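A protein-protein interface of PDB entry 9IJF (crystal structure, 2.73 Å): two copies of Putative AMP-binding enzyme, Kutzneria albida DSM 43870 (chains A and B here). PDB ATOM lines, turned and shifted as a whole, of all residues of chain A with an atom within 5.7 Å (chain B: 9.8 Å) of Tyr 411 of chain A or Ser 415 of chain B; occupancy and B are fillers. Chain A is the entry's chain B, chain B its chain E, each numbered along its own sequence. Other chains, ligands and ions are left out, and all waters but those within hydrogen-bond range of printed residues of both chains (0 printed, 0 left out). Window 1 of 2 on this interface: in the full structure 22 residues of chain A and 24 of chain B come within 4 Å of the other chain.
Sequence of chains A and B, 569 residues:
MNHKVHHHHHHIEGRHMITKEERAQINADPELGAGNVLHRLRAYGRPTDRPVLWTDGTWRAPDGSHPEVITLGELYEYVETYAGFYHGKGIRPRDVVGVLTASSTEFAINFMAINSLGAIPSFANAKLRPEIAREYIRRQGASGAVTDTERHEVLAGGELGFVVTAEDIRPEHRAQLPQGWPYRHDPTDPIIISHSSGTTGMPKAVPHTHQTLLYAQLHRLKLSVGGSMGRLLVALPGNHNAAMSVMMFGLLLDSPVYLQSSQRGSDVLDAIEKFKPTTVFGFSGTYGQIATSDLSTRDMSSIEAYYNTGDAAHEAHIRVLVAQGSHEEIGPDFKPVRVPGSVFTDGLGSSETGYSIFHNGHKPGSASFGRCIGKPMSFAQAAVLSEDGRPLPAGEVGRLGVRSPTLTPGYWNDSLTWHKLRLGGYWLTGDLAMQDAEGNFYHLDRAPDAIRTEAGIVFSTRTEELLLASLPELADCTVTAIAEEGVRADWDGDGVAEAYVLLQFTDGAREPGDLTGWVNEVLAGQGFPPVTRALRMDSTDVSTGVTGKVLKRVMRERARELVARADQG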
ATOM      1  N   LYS A 204       0.393   5.753  -5.442  1.00  0.00           N
ATOM      2  CA  LYS A 204      -0.273   6.252  -6.636  1.00  0.00           C
ATOM      3  C   LYS A 204      -1.356   7.245  -6.236  1.00  0.00           C
ATOM      4  O   LYS A 204      -2.203   6.942  -5.378  1.00  0.00           O
ATOM      5  CB  LYS A 204      -0.864   5.098  -7.435  1.00  0.00           C
ATOM      6  CG  LYS A 204       0.199   4.123  -7.926  1.00  0.00           C
ATOM      7  CD  LYS A 204      -0.396   3.039  -8.832  1.00  0.00           C
ATOM      8  CE  LYS A 204      -1.378   2.169  -8.088  1.00  0.00           C
ATOM      9  NZ  LYS A 204      -0.788   0.826  -7.867  1.00  0.00           N
ATOM     10  N   ALA A 205      -1.319   8.433  -6.841  1.00  0.00           N
ATOM     11  CA  ALA A 205      -2.312   9.456  -6.539  1.00  0.00           C
ATOM     12  C   ALA A 205      -3.631   9.127  -7.252  1.00  0.00           C
ATOM     13  O   ALA A 205      -3.665   8.955  -8.478  1.00  0.00           O
ATOM     14  CB  ALA A 205      -1.784  10.832  -6.943  1.00  0.00           C
ATOM     15  N   VAL A 206      -4.715   9.017  -6.493  1.00  0.00           N
ATOM     16  CA  VAL A 206      -6.007   8.620  -7.040  1.00  0.00           C
ATOM     17  C   VAL A 206      -6.950   9.815  -6.910  1.00  0.00           C
ATOM     18  O   VAL A 206      -7.359  10.171  -5.790  1.00  0.00           O
ATOM     19  CB  VAL A 206      -6.574   7.380  -6.336  1.00  0.00           C
ATOM     20  CG1 VAL A 206      -7.948   7.062  -6.869  1.00  0.00           C
ATOM     21  CG2 VAL A 206      -5.654   6.188  -6.529  1.00  0.00           C
ATOM     22  N   PRO A 207      -7.286  10.491  -8.001  1.00  0.00           N
ATOM     23  CA  PRO A 207      -8.289  11.557  -7.917  1.00  0.00           C
ATOM     24  C   PRO A 207      -9.702  10.986  -7.916  1.00  0.00           C
ATOM     25  O   PRO A 207      -9.979   9.921  -8.476  1.00  0.00           O
ATOM     26  CB  PRO A 207      -8.029  12.397  -9.172  1.00  0.00           C
ATOM     27  CG  PRO A 207      -7.311  11.456 -10.115  1.00  0.00           C
ATOM     28  CD  PRO A 207      -6.713  10.333  -9.352  1.00  0.00           C
ATOM     29  N   GLU A 352      -9.290   3.372  -5.742  1.00  0.00           N
ATOM     30  CA  GLU A 352      -9.744   3.555  -7.122  1.00  0.00           C
ATOM     31  C   GLU A 352     -11.251   3.365  -7.251  1.00  0.00           C
ATOM     32  O   GLU A 352     -11.952   4.262  -7.721  1.00  0.00           O
ATOM     33  CB  GLU A 352      -9.011   2.598  -8.061  1.00  0.00           C
ATOM     34  CG  GLU A 352      -7.524   2.834  -8.159  1.00  0.00           C
ATOM     35  CD  GLU A 352      -6.752   2.098  -7.082  1.00  0.00           C
ATOM     36  OE1 GLU A 352      -7.334   1.890  -5.992  1.00  0.00           O
ATOM     37  OE2 GLU A 352      -5.573   1.715  -7.340  1.00  0.00           O
ATOM     38  N   THR A 408     -12.250   5.949 -10.525  1.00  0.00           N
ATOM     39  CA  THR A 408     -11.517   7.171 -10.775  1.00  0.00           C
ATOM     40  C   THR A 408     -11.287   7.352 -12.273  1.00  0.00           C
ATOM     41  O   THR A 408     -11.271   6.383 -13.040  1.00  0.00           O
ATOM     42  CB  THR A 408     -10.170   7.169 -10.056  1.00  0.00           C
ATOM     43  OG1 THR A 408      -9.397   8.293 -10.517  1.00  0.00           O
ATOM     44  CG2 THR A 408      -9.417   5.865 -10.331  1.00  0.00           C
ATOM     45  N   PRO A 409     -11.126   8.593 -12.720  1.00  0.00           N
ATOM     46  CA  PRO A 409     -10.653   8.825 -14.092  1.00  0.00           C
ATOM     47  C   PRO A 409      -9.205   8.431 -14.314  1.00  0.00           C
ATOM     48  O   PRO A 409      -8.791   8.318 -15.471  1.00  0.00           O
ATOM     49  CB  PRO A 409     -10.869  10.325 -14.288  1.00  0.00           C
ATOM     50  CG  PRO A 409     -11.024  10.883 -12.882  1.00  0.00           C
ATOM     51  CD  PRO A 409     -11.644   9.815 -12.077  1.00  0.00           C
ATOM     52  N   GLY A 410      -8.427   8.199 -13.274  1.00  0.00           N
ATOM     53  CA  GLY A 410      -7.100   7.635 -13.442  1.00  0.00           C
ATOM     54  C   GLY A 410      -6.042   8.352 -12.624  1.00  0.00           C
ATOM     55  O   GLY A 410      -6.217   9.491 -12.200  1.00  0.00           O
ATOM     56  N   TYR A 411      -4.914   7.657 -12.409  1.00  0.00           N
ATOM     57  CA  TYR A 411      -3.904   8.110 -11.461  1.00  0.00           C
ATOM     58  C   TYR A 411      -3.387   9.478 -11.881  1.00  0.00           C
ATOM     59  O   TYR A 411      -3.158   9.738 -13.070  1.00  0.00           O
ATOM     60  CB  TYR A 411      -2.763   7.093 -11.371  1.00  0.00           C
ATOM     61  CG  TYR A 411      -3.231   5.719 -10.941  1.00  0.00           C
ATOM     62  CD1 TYR A 411      -4.021   5.559  -9.791  1.00  0.00           C
ATOM     63  CD2 TYR A 411      -2.919   4.575 -11.692  1.00  0.00           C
ATOM     64  CE1 TYR A 411      -4.476   4.300  -9.390  1.00  0.00           C
ATOM     65  CE2 TYR A 411      -3.372   3.309 -11.296  1.00  0.00           C
ATOM     66  CZ  TYR A 411      -4.148   3.186 -10.142  1.00  0.00           C
ATOM     67  OH  TYR A 411      -4.599   1.954  -9.729  1.00  0.00           O
ATOM     68  N   TRP A 412      -3.253  10.367 -10.893  1.00  0.00           N
ATOM     69  CA  TRP A 412      -2.928  11.762 -11.150  1.00  0.00           C
ATOM     70  C   TRP A 412      -1.490  11.867 -11.656  1.00  0.00           C
ATOM     71  O   TRP A 412      -0.566  11.294 -11.071  1.00  0.00           O
ATOM     72  CB  TRP A 412      -3.149  12.586  -9.878  1.00  0.00           C
ATOM     73  CG  TRP A 412      -3.080  14.089 -10.050  1.00  0.00           C
ATOM     74  CD1 TRP A 412      -1.981  14.889  -9.841  1.00  0.00           C
ATOM     75  CD2 TRP A 412      -4.146  14.977 -10.449  1.00  0.00           C
ATOM     76  NE1 TRP A 412      -2.296  16.201 -10.084  1.00  0.00           N
ATOM     77  CE2 TRP A 412      -3.612  16.288 -10.465  1.00  0.00           C
ATOM     78  CE3 TRP A 412      -5.490  14.795 -10.801  1.00  0.00           C
ATOM     79  CZ2 TRP A 412      -4.378  17.408 -10.814  1.00  0.00           C
ATOM     80  CZ3 TRP A 412      -6.251  15.919 -11.165  1.00  0.00           C
ATOM     81  CH2 TRP A 412      -5.693  17.201 -11.160  1.00  0.00           C
ATOM     82  N   ASN A 413      -1.329  12.556 -12.782  1.00  0.00           N
ATOM     83  CA  ASN A 413      -0.054  12.715 -13.493  1.00  0.00           C
ATOM     84  C   ASN A 413       0.659  11.378 -13.692  1.00  0.00           C
ATOM     85  O   ASN A 413       1.891  11.297 -13.658  1.00  0.00           O
ATOM     86  CB  ASN A 413       0.860  13.731 -12.791  1.00  0.00           C
ATOM     87  CG  ASN A 413       0.308  15.150 -12.838  1.00  0.00           C
ATOM     88  OD1 ASN A 413      -0.511  15.481 -13.698  1.00  0.00           O
ATOM     89  ND2 ASN A 413       0.768  16.001 -11.915  1.00  0.00           N
ATOM     90  N   ASP A 414      -0.120  10.312 -13.917  1.00  0.00           N
ATOM     91  CA  ASP A 414       0.539   9.047 -14.248  1.00  0.00           C
ATOM     92  C   ASP A 414      -0.414   8.227 -15.122  1.00  0.00           C
ATOM     93  O   ASP A 414      -1.038   7.259 -14.685  1.00  0.00           O
ATOM     94  CB  ASP A 414       0.969   8.273 -13.003  1.00  0.00           C
ATOM     95  CG  ASP A 414       1.919   7.117 -13.320  1.00  0.00           C
ATOM     96  OD1 ASP A 414       2.412   7.000 -14.480  1.00  0.00           O
ATOM     97  OD2 ASP A 414       2.167   6.328 -12.378  1.00  0.00           O
ATOM     98  N   SER A 415      -0.502   8.631 -16.386  1.00  0.00           N
ATOM     99  CA  SER A 415      -1.220   7.854 -17.383  1.00  0.00           C
ATOM    100  C   SER A 415      -0.571   6.494 -17.597  1.00  0.00           C
ATOM    101  O   SER A 415      -1.274   5.481 -17.730  1.00  0.00           O
ATOM    102  CB  SER A 415      -1.263   8.624 -18.702  1.00  0.00           C
ATOM    103  OG  SER A 415      -1.745   9.948 -18.516  1.00  0.00           O
ATOM    104  N   THR A 417       0.949   4.342 -15.765  1.00  0.00           N
ATOM    105  CA  THR A 417       0.546   3.293 -14.835  1.00  0.00           C
ATOM    106  C   THR A 417      -0.951   2.996 -14.951  1.00  0.00           C
ATOM    107  O   THR A 417      -1.354   1.829 -15.032  1.00  0.00           O
ATOM    108  CB  THR A 417       0.933   3.706 -13.413  1.00  0.00           C
ATOM    109  OG1 THR A 417       2.352   3.876 -13.365  1.00  0.00           O
ATOM    110  CG2 THR A 417       0.470   2.693 -12.339  1.00  0.00           C
ATOM    111  N   TRP A 418      -1.780   4.043 -14.977  1.00  0.00           N
ATOM    112  CA  TRP A 418      -3.223   3.853 -15.109  1.00  0.00           C
ATOM    113  C   TRP A 418      -3.583   2.883 -16.232  1.00  0.00           C
ATOM    114  O   TRP A 418      -4.438   2.015 -16.055  1.00  0.00           O
ATOM    115  CB  TRP A 418      -3.918   5.199 -15.329  1.00  0.00           C
ATOM    116  CG  TRP A 418      -5.406   5.118 -15.536  1.00  0.00           C
ATOM    117  CD1 TRP A 418      -6.098   5.493 -16.654  1.00  0.00           C
ATOM    118  CD2 TRP A 418      -6.391   4.653 -14.594  1.00  0.00           C
ATOM    119  NE1 TRP A 418      -7.456   5.311 -16.458  1.00  0.00           N
ATOM    120  CE2 TRP A 418      -7.659   4.792 -15.207  1.00  0.00           C
ATOM    121  CE3 TRP A 418      -6.330   4.159 -13.286  1.00  0.00           C
ATOM    122  CZ2 TRP A 418      -8.841   4.431 -14.567  1.00  0.00           C
ATOM    123  CZ3 TRP A 418      -7.508   3.806 -12.651  1.00  0.00           C
ATOM    124  CH2 TRP A 418      -8.750   3.943 -13.291  1.00  0.00           C
ATOM    125  N   LEU A 421      -2.854  -0.785 -15.668  1.00  0.00           N
ATOM    126  CA  LEU A 421      -3.774  -1.397 -14.728  1.00  0.00           C
ATOM    127  C   LEU A 421      -5.197  -1.454 -15.283  1.00  0.00           C
ATOM    128  O   LEU A 421      -6.163  -1.561 -14.514  1.00  0.00           O
ATOM    129  CB  LEU A 421      -3.708  -0.658 -13.385  1.00  0.00           C
ATOM    130  CG  LEU A 421      -2.664  -1.281 -12.433  1.00  0.00           C
ATOM    131  CD1 LEU A 421      -1.316  -1.539 -13.088  1.00  0.00           C
ATOM    132  CD2 LEU A 421      -2.468  -0.480 -11.169  1.00  0.00           C
ATOM    133  N   TRP A 427     -10.808  -1.839 -14.962  1.00  0.00           N
ATOM    134  CA  TRP A 427      -9.643  -1.549 -14.137  1.00  0.00           C
ATOM    135  C   TRP A 427      -9.244  -2.816 -13.373  1.00  0.00           C
ATOM    136  O   TRP A 427     -10.045  -3.358 -12.607  1.00  0.00           O
ATOM    137  CB  TRP A 427      -9.947  -0.387 -13.185  1.00  0.00           C
ATOM    138  CG  TRP A 427      -8.863  -0.162 -12.174  1.00  0.00           C
ATOM    139  CD1 TRP A 427      -7.649   0.452 -12.375  1.00  0.00           C
ATOM    140  CD2 TRP A 427      -8.876  -0.580 -10.811  1.00  0.00           C
ATOM    141  NE1 TRP A 427      -6.923   0.456 -11.213  1.00  0.00           N
ATOM    142  CE2 TRP A 427      -7.652  -0.173 -10.236  1.00  0.00           C
ATOM    143  CE3 TRP A 427      -9.815  -1.246 -10.010  1.00  0.00           C
ATOM    144  CZ2 TRP A 427      -7.335  -0.429  -8.905  1.00  0.00           C
ATOM    145  CZ3 TRP A 427      -9.500  -1.488  -8.682  1.00  0.00           C
ATOM    146  CH2 TRP A 427      -8.267  -1.085  -8.145  1.00  0.00           C
ATOM    147  N   LYS B 204       2.211  19.846 -25.247  1.00  0.00           N
ATOM    148  CA  LYS B 204       1.364  18.962 -24.472  1.00  0.00           C
ATOM    149  C   LYS B 204       1.006  17.713 -25.261  1.00  0.00           C
ATOM    150  O   LYS B 204       0.640  17.779 -26.447  1.00  0.00           O
ATOM    151  CB  LYS B 204       0.122  19.693 -23.970  1.00  0.00           C
ATOM    152  CG  LYS B 204       0.366  20.224 -22.558  1.00  0.00           C
ATOM    153  CD  LYS B 204       1.559  19.459 -21.818  1.00  0.00           C
ATOM    154  CE  LYS B 204       1.156  18.116 -21.145  1.00  0.00           C
ATOM    155  NZ  LYS B 204       1.748  16.840 -21.717  1.00  0.00           N
ATOM    156  N   ALA B 205       1.121  16.577 -24.561  1.00  0.00           N
ATOM    157  CA  ALA B 205       1.051  15.228 -25.111  1.00  0.00           C
ATOM    158  C   ALA B 205      -0.395  14.721 -25.082  1.00  0.00           C
ATOM    159  O   ALA B 205      -1.014  14.616 -24.007  1.00  0.00           O
ATOM    160  CB  ALA B 205       1.978  14.306 -24.315  1.00  0.00           C
ATOM    161  N   PRO B 207      -2.956  11.756 -26.007  1.00  0.00           N
ATOM    162  CA  PRO B 207      -3.276  10.394 -26.408  1.00  0.00           C
ATOM    163  C   PRO B 207      -4.622  10.316 -27.104  1.00  0.00           C
ATOM    164  O   PRO B 207      -5.542  11.104 -26.843  1.00  0.00           O
ATOM    165  CB  PRO B 207      -3.310   9.640 -25.076  1.00  0.00           C
ATOM    166  CG  PRO B 207      -3.715  10.658 -24.100  1.00  0.00           C
ATOM    167  CD  PRO B 207      -3.319  12.002 -24.604  1.00  0.00           C
ATOM    168  N   PRO B 409      -8.763  11.392 -23.776  1.00  0.00           N
ATOM    169  CA  PRO B 409      -9.058  11.176 -22.353  1.00  0.00           C
ATOM    170  C   PRO B 409      -8.261  12.065 -21.405  1.00  0.00           C
ATOM    171  O   PRO B 409      -8.569  12.079 -20.203  1.00  0.00           O
ATOM    172  CB  PRO B 409      -8.730   9.695 -22.156  1.00  0.00           C
ATOM    173  CG  PRO B 409      -7.760   9.369 -23.268  1.00  0.00           C
ATOM    174  CD  PRO B 409      -8.121  10.226 -24.416  1.00  0.00           C
ATOM    175  N   GLY B 410      -7.284  12.822 -21.891  1.00  0.00           N
ATOM    176  CA  GLY B 410      -6.504  13.728 -21.061  1.00  0.00           C
ATOM    177  C   GLY B 410      -5.042  13.773 -21.483  1.00  0.00           C
ATOM    178  O   GLY B 410      -4.529  12.887 -22.157  1.00  0.00           O
ATOM    179  N   TYR B 411      -4.350  14.835 -21.074  1.00  0.00           N
ATOM    180  CA  TYR B 411      -2.939  14.972 -21.434  1.00  0.00           C
ATOM    181  C   TYR B 411      -2.126  13.864 -20.765  1.00  0.00           C
ATOM    182  O   TYR B 411      -2.292  13.582 -19.573  1.00  0.00           O
ATOM    183  CB  TYR B 411      -2.424  16.364 -21.052  1.00  0.00           C
ATOM    184  CG  TYR B 411      -3.110  17.446 -21.859  1.00  0.00           C
ATOM    185  CD1 TYR B 411      -3.198  17.340 -23.246  1.00  0.00           C
ATOM    186  CD2 TYR B 411      -3.702  18.548 -21.252  1.00  0.00           C
ATOM    187  CE1 TYR B 411      -3.836  18.300 -24.011  1.00  0.00           C
ATOM    188  CE2 TYR B 411      -4.340  19.523 -22.014  1.00  0.00           C
ATOM    189  CZ  TYR B 411      -4.405  19.386 -23.394  1.00  0.00           C
ATOM    190  OH  TYR B 411      -5.047  20.321 -24.187  1.00  0.00           O
ATOM    191  N   TRP B 412      -1.269  13.211 -21.556  1.00  0.00           N
ATOM    192  CA  TRP B 412      -0.421  12.146 -21.035  1.00  0.00           C
ATOM    193  C   TRP B 412       0.411  12.633 -19.855  1.00  0.00           C
ATOM    194  O   TRP B 412       1.099  13.656 -19.932  1.00  0.00           O
ATOM    195  CB  TRP B 412       0.494  11.615 -22.133  1.00  0.00           C
ATOM    196  CG  TRP B 412       1.115  10.314 -21.778  1.00  0.00           C
ATOM    197  CD1 TRP B 412       2.396  10.108 -21.410  1.00  0.00           C
ATOM    198  CD2 TRP B 412       0.476   9.026 -21.758  1.00  0.00           C
ATOM    199  NE1 TRP B 412       2.610   8.783 -21.164  1.00  0.00           N
ATOM    200  CE2 TRP B 412       1.451   8.093 -21.369  1.00  0.00           C
ATOM    201  CE3 TRP B 412      -0.828   8.574 -22.044  1.00  0.00           C
ATOM    202  CZ2 TRP B 412       1.179   6.737 -21.237  1.00  0.00           C
ATOM    203  CZ3 TRP B 412      -1.111   7.227 -21.915  1.00  0.00           C
ATOM    204  CH2 TRP B 412      -0.110   6.319 -21.516  1.00  0.00           C
ATOM    205  N   ASN B 413       0.302  11.900 -18.754  1.00  0.00           N
ATOM    206  CA  ASN B 413       1.040  12.129 -17.518  1.00  0.00           C
ATOM    207  C   ASN B 413       0.927  13.567 -17.045  1.00  0.00           C
ATOM    208  O   ASN B 413       1.788  14.067 -16.321  1.00  0.00           O
ATOM    209  CB  ASN B 413       2.498  11.706 -17.664  1.00  0.00           C
ATOM    210  CG  ASN B 413       2.648  10.202 -17.766  1.00  0.00           C
ATOM    211  OD1 ASN B 413       1.729   9.487 -17.402  1.00  0.00           O
ATOM    212  ND2 ASN B 413       3.807   9.714 -18.247  1.00  0.00           N
ATOM    213  N   ASP B 414      -0.156  14.252 -17.402  1.00  0.00           N
ATOM    214  CA  ASP B 414      -0.297  15.641 -16.984  1.00  0.00           C
ATOM    215  C   ASP B 414      -1.773  15.943 -16.729  1.00  0.00           C
ATOM    216  O   ASP B 414      -2.397  16.752 -17.396  1.00  0.00           O
ATOM    217  CB  ASP B 414       0.321  16.596 -18.009  1.00  0.00           C
ATOM    218  CG  ASP B 414       0.417  18.001 -17.488  1.00  0.00           C
ATOM    219  OD1 ASP B 414       0.076  18.197 -16.291  1.00  0.00           O
ATOM    220  OD2 ASP B 414       0.808  18.891 -18.286  1.00  0.00           O
ATOM    221  N   SER B 415      -2.313  15.282 -15.709  1.00  0.00           N
ATOM    222  CA  SER B 415      -3.664  15.546 -15.245  1.00  0.00           C
ATOM    223  C   SER B 415      -3.853  16.990 -14.807  1.00  0.00           C
ATOM    224  O   SER B 415      -4.977  17.502 -14.842  1.00  0.00           O
ATOM    225  CB  SER B 415      -3.983  14.608 -14.090  1.00  0.00           C
ATOM    226  OG  SER B 415      -3.396  13.346 -14.335  1.00  0.00           O
ATOM    227  N   LEU B 416      -2.789  17.657 -14.355  1.00  0.00           N
ATOM    228  CA  LEU B 416      -2.940  19.018 -13.834  1.00  0.00           C
ATOM    229  C   LEU B 416      -3.301  19.993 -14.956  1.00  0.00           C
ATOM    230  O   LEU B 416      -4.272  20.755 -14.859  1.00  0.00           O
ATOM    231  CB  LEU B 416      -1.647  19.443 -13.135  1.00  0.00           C
ATOM    232  CG  LEU B 416      -1.584  20.817 -12.467  1.00  0.00           C
ATOM    233  CD1 LEU B 416      -2.462  20.829 -11.225  1.00  0.00           C
ATOM    234  CD2 LEU B 416      -0.158  21.179 -12.111  1.00  0.00           C
ATOM    235  N   THR B 417      -2.543  19.955 -16.047  1.00  0.00           N
ATOM    236  CA  THR B 417      -2.846  20.823 -17.173  1.00  0.00           C
ATOM    237  C   THR B 417      -4.180  20.447 -17.797  1.00  0.00           C
ATOM    238  O   THR B 417      -4.928  21.319 -18.258  1.00  0.00           O
ATOM    239  CB  THR B 417      -1.719  20.732 -18.196  1.00  0.00           C
ATOM    240  OG1 THR B 417      -0.501  21.087 -17.550  1.00  0.00           O
ATOM    241  CG2 THR B 417      -1.961  21.632 -19.389  1.00  0.00           C
ATOM    242  N   TRP B 418      -4.491  19.152 -17.818  1.00  0.00           N
ATOM    243  CA  TRP B 418      -5.723  18.699 -18.439  1.00  0.00           C
ATOM    244  C   TRP B 418      -6.925  19.327 -17.760  1.00  0.00           C
ATOM    245  O   TRP B 418      -7.817  19.864 -18.426  1.00  0.00           O
ATOM    246  CB  TRP B 418      -5.789  17.182 -18.388  1.00  0.00           C
ATOM    247  CG  TRP B 418      -7.073  16.590 -18.889  1.00  0.00           C
ATOM    248  CD1 TRP B 418      -7.919  15.773 -18.192  1.00  0.00           C
ATOM    249  CD2 TRP B 418      -7.642  16.735 -20.201  1.00  0.00           C
ATOM    250  NE1 TRP B 418      -8.979  15.397 -18.988  1.00  0.00           N
ATOM    251  CE2 TRP B 418      -8.835  15.966 -20.226  1.00  0.00           C
ATOM    252  CE3 TRP B 418      -7.255  17.425 -21.361  1.00  0.00           C
ATOM    253  CZ2 TRP B 418      -9.657  15.884 -21.357  1.00  0.00           C
ATOM    254  CZ3 TRP B 418      -8.069  17.330 -22.501  1.00  0.00           C
ATOM    255  CH2 TRP B 418      -9.264  16.568 -22.482  1.00  0.00           C
ATOM    256  N   HIS B 419      -6.958  19.307 -16.434  1.00  0.00           N
ATOM    257  CA  HIS B 419      -8.142  19.869 -15.804  1.00  0.00           C
ATOM    258  C   HIS B 419      -8.127  21.387 -15.779  1.00  0.00           C
ATOM    259  O   HIS B 419      -9.177  22.007 -15.558  1.00  0.00           O
ATOM    260  CB  HIS B 419      -8.318  19.295 -14.412  1.00  0.00           C
ATOM    261  CG  HIS B 419      -8.776  17.874 -14.435  1.00  0.00           C
ATOM    262  ND1 HIS B 419     -10.104  17.526 -14.549  1.00  0.00           N
ATOM    263  CD2 HIS B 419      -8.080  16.712 -14.417  1.00  0.00           C
ATOM    264  CE1 HIS B 419     -10.209  16.209 -14.567  1.00  0.00           C
ATOM    265  NE2 HIS B 419      -8.994  15.692 -14.490  1.00  0.00           N
ATOM    266  N   LYS B 420      -6.977  22.000 -16.048  1.00  0.00           N
ATOM    267  CA  LYS B 420      -6.980  23.433 -16.240  1.00  0.00           C
ATOM    268  C   LYS B 420      -7.570  23.827 -17.584  1.00  0.00           C
ATOM    269  O   LYS B 420      -7.987  24.971 -17.732  1.00  0.00           O
ATOM    270  CB  LYS B 420      -5.573  23.977 -16.092  1.00  0.00           C
ATOM    271  CG  LYS B 420      -5.122  24.127 -14.668  1.00  0.00           C
ATOM    272  CD  LYS B 420      -3.638  24.377 -14.718  1.00  0.00           C
ATOM    273  CE  LYS B 420      -2.926  24.397 -13.394  1.00  0.00           C
ATOM    274  NZ  LYS B 420      -1.494  24.656 -13.761  1.00  0.00           N
ATOM    275  N   LEU B 421      -7.632  22.918 -18.563  1.00  0.00           N
ATOM    276  CA  LEU B 421      -8.231  23.239 -19.852  1.00  0.00           C
ATOM    277  C   LEU B 421      -9.662  22.691 -19.970  1.00  0.00           C
ATOM    278  O   LEU B 421     -10.196  22.540 -21.082  1.00  0.00           O
ATOM    279  CB  LEU B 421      -7.329  22.756 -20.994  1.00  0.00           C
ATOM    280  CG  LEU B 421      -5.929  23.400 -20.898  1.00  0.00           C
ATOM    281  CD1 LEU B 421      -5.026  23.101 -22.074  1.00  0.00           C
ATOM    282  CD2 LEU B 421      -6.034  24.896 -20.724  1.00  0.00           C
ATOM    283  N   ARG B 422     -10.309  22.441 -18.833  1.00  0.00           N
ATOM    284  CA  ARG B 422     -11.676  21.975 -18.791  1.00  0.00           C
ATOM    285  C   ARG B 422     -12.486  22.911 -17.908  1.00  0.00           C
ATOM    286  O   ARG B 422     -11.976  23.459 -16.919  1.00  0.00           O
ATOM    287  CB  ARG B 422     -11.763  20.545 -18.261  1.00  0.00           C
ATOM    288  CG  ARG B 422     -11.198  19.471 -19.177  1.00  0.00           C
ATOM    289  CD  ARG B 422     -11.220  18.137 -18.489  1.00  0.00           C
ATOM    290  NE  ARG B 422     -12.475  17.972 -17.773  1.00  0.00           N
ATOM    291  CZ  ARG B 422     -13.532  17.338 -18.262  1.00  0.00           C
ATOM    292  NH1 ARG B 422     -13.499  16.747 -19.449  1.00  0.00           N
ATOM    293  NH2 ARG B 422     -14.644  17.282 -17.540  1.00  0.00           N
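Ser 415 of chain B touches Tyr 411 of chain A. CA of Trp 412 of chain A touches OG of Ser 415 of chain B (3.6 Å). Trp 412 of chain A touches His 419 of chain B. Asn 413 of chain A touches Asn 413 of chain B (CA to O, 3.6 Å). Asp 414 of chain A touches Asn 413 of chain B (C to OD1, 3.4 Å). Ser 415 of chain A touches Tyr 411 of chain B (OG to O, 3.8 Å). CB of Ser 415 of chain A touches CE3 of Trp 412 of chain B, at 3.4 Å.
The side-chain hydroxyl (OG) of Ser 415 of chain B is in hydrogen-bond range of the backbone NH (N) of Asn 413 of chain A. OD1 of Asn 413 of chain A is in hydrogen-bond range of N of Leu 416 of chain B. The side-chain amide oxygen of Asn 413 of chain B is in hydrogen-bond range of the backbone NH of Ser 415 of chain A (2.6 Å).
Tyr 411 of chain A touches Ser 415 of chain B, and with the chains exchanged Ser 415 of chain A touches Tyr 411 of chain B. Trp 412 of chain A touches Ser 415 of chain B, and with the chains exchanged Ser 415 of chain A touches Trp 412 of chain B. Of the 12 pairs that touch across the chains among the printed residues, 9 have their exchanged pair printed and touching as well.
Of the 17 printed residues of chain A, 5 touch a printed residue of chain B. Printed residues of chain A that touch a printed residue of chain B: Tyr 411, Trp 412, Asn 413, Asp 414 and Ser 415. Printed residues of chain B that touch a printed residue of chain A: Tyr 411, Trp 412, Asn 413, Asp 414, Ser 415, Leu 416 and His 419. Hydrophobic or aromatic side chains of chain B that line the printed part of chain A: Trp 412, Leu 416 and His 419. Among the printed residues, 12 pairs touch across the chains. Among the printed residues, no Asp or Glu carboxylate lies within 4 Å of a Lys or Arg side-chain nitrogen of the other chain.
Of chain B, only Ser 415 (3.8 Å) comes within 4 Å of Tyr 411 of chain A. Of chain A, only Tyr 411 (3.8 Å), Trp 412 (3.6 Å) and Asn 413 (2.7 Å) come within 4 Å of Ser 415 of chain B. Ala 205 of chain A touches none of the printed residues of chain B. No residue of chain B comes within 4 Å of Gly 410 of chain A. Trp 412 of chain A touches three residues of chain B. No residue of chain B comes within 4 Å of Trp 418 of chain A. Printed residues of chain A within 4 Å of His 419 of chain B: Trp 412. Printed residues of chain B within 4 Å of Asp 414 of chain A: Asn 413. Of the printed residues of chain A, Asp 414 of chain B touches Asn 413. Pro 409 of chain A touches none of the printed residues of chain B. The nearest residue of chain A that does not touch Ser 415 of chain B is Asp 414 of chain A (4.5 Å). The nearest printed residue of chain B that does not touch Ser 415 of chain A is Asp 414 of chain B (4.7 Å).
OD1 of Asp 414 of chain B lies close to N of Leu 416 of chain B (3.5 Å). The side-chain hydroxyl of Tyr 411 of chain A lies within hydrogen-bond range of the indole nitrogen of Trp 427 of chain A (3.1 Å). O of Ala 205 of chain A is in hydrogen-bond range of N of Trp 412 of chain A (2.8 Å). The indole nitrogen (NE1) of Trp 412 of chain B lies close to the side-chain amide nitrogen (ND2) of Asn 413 of chain B, at 3.3 Å.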
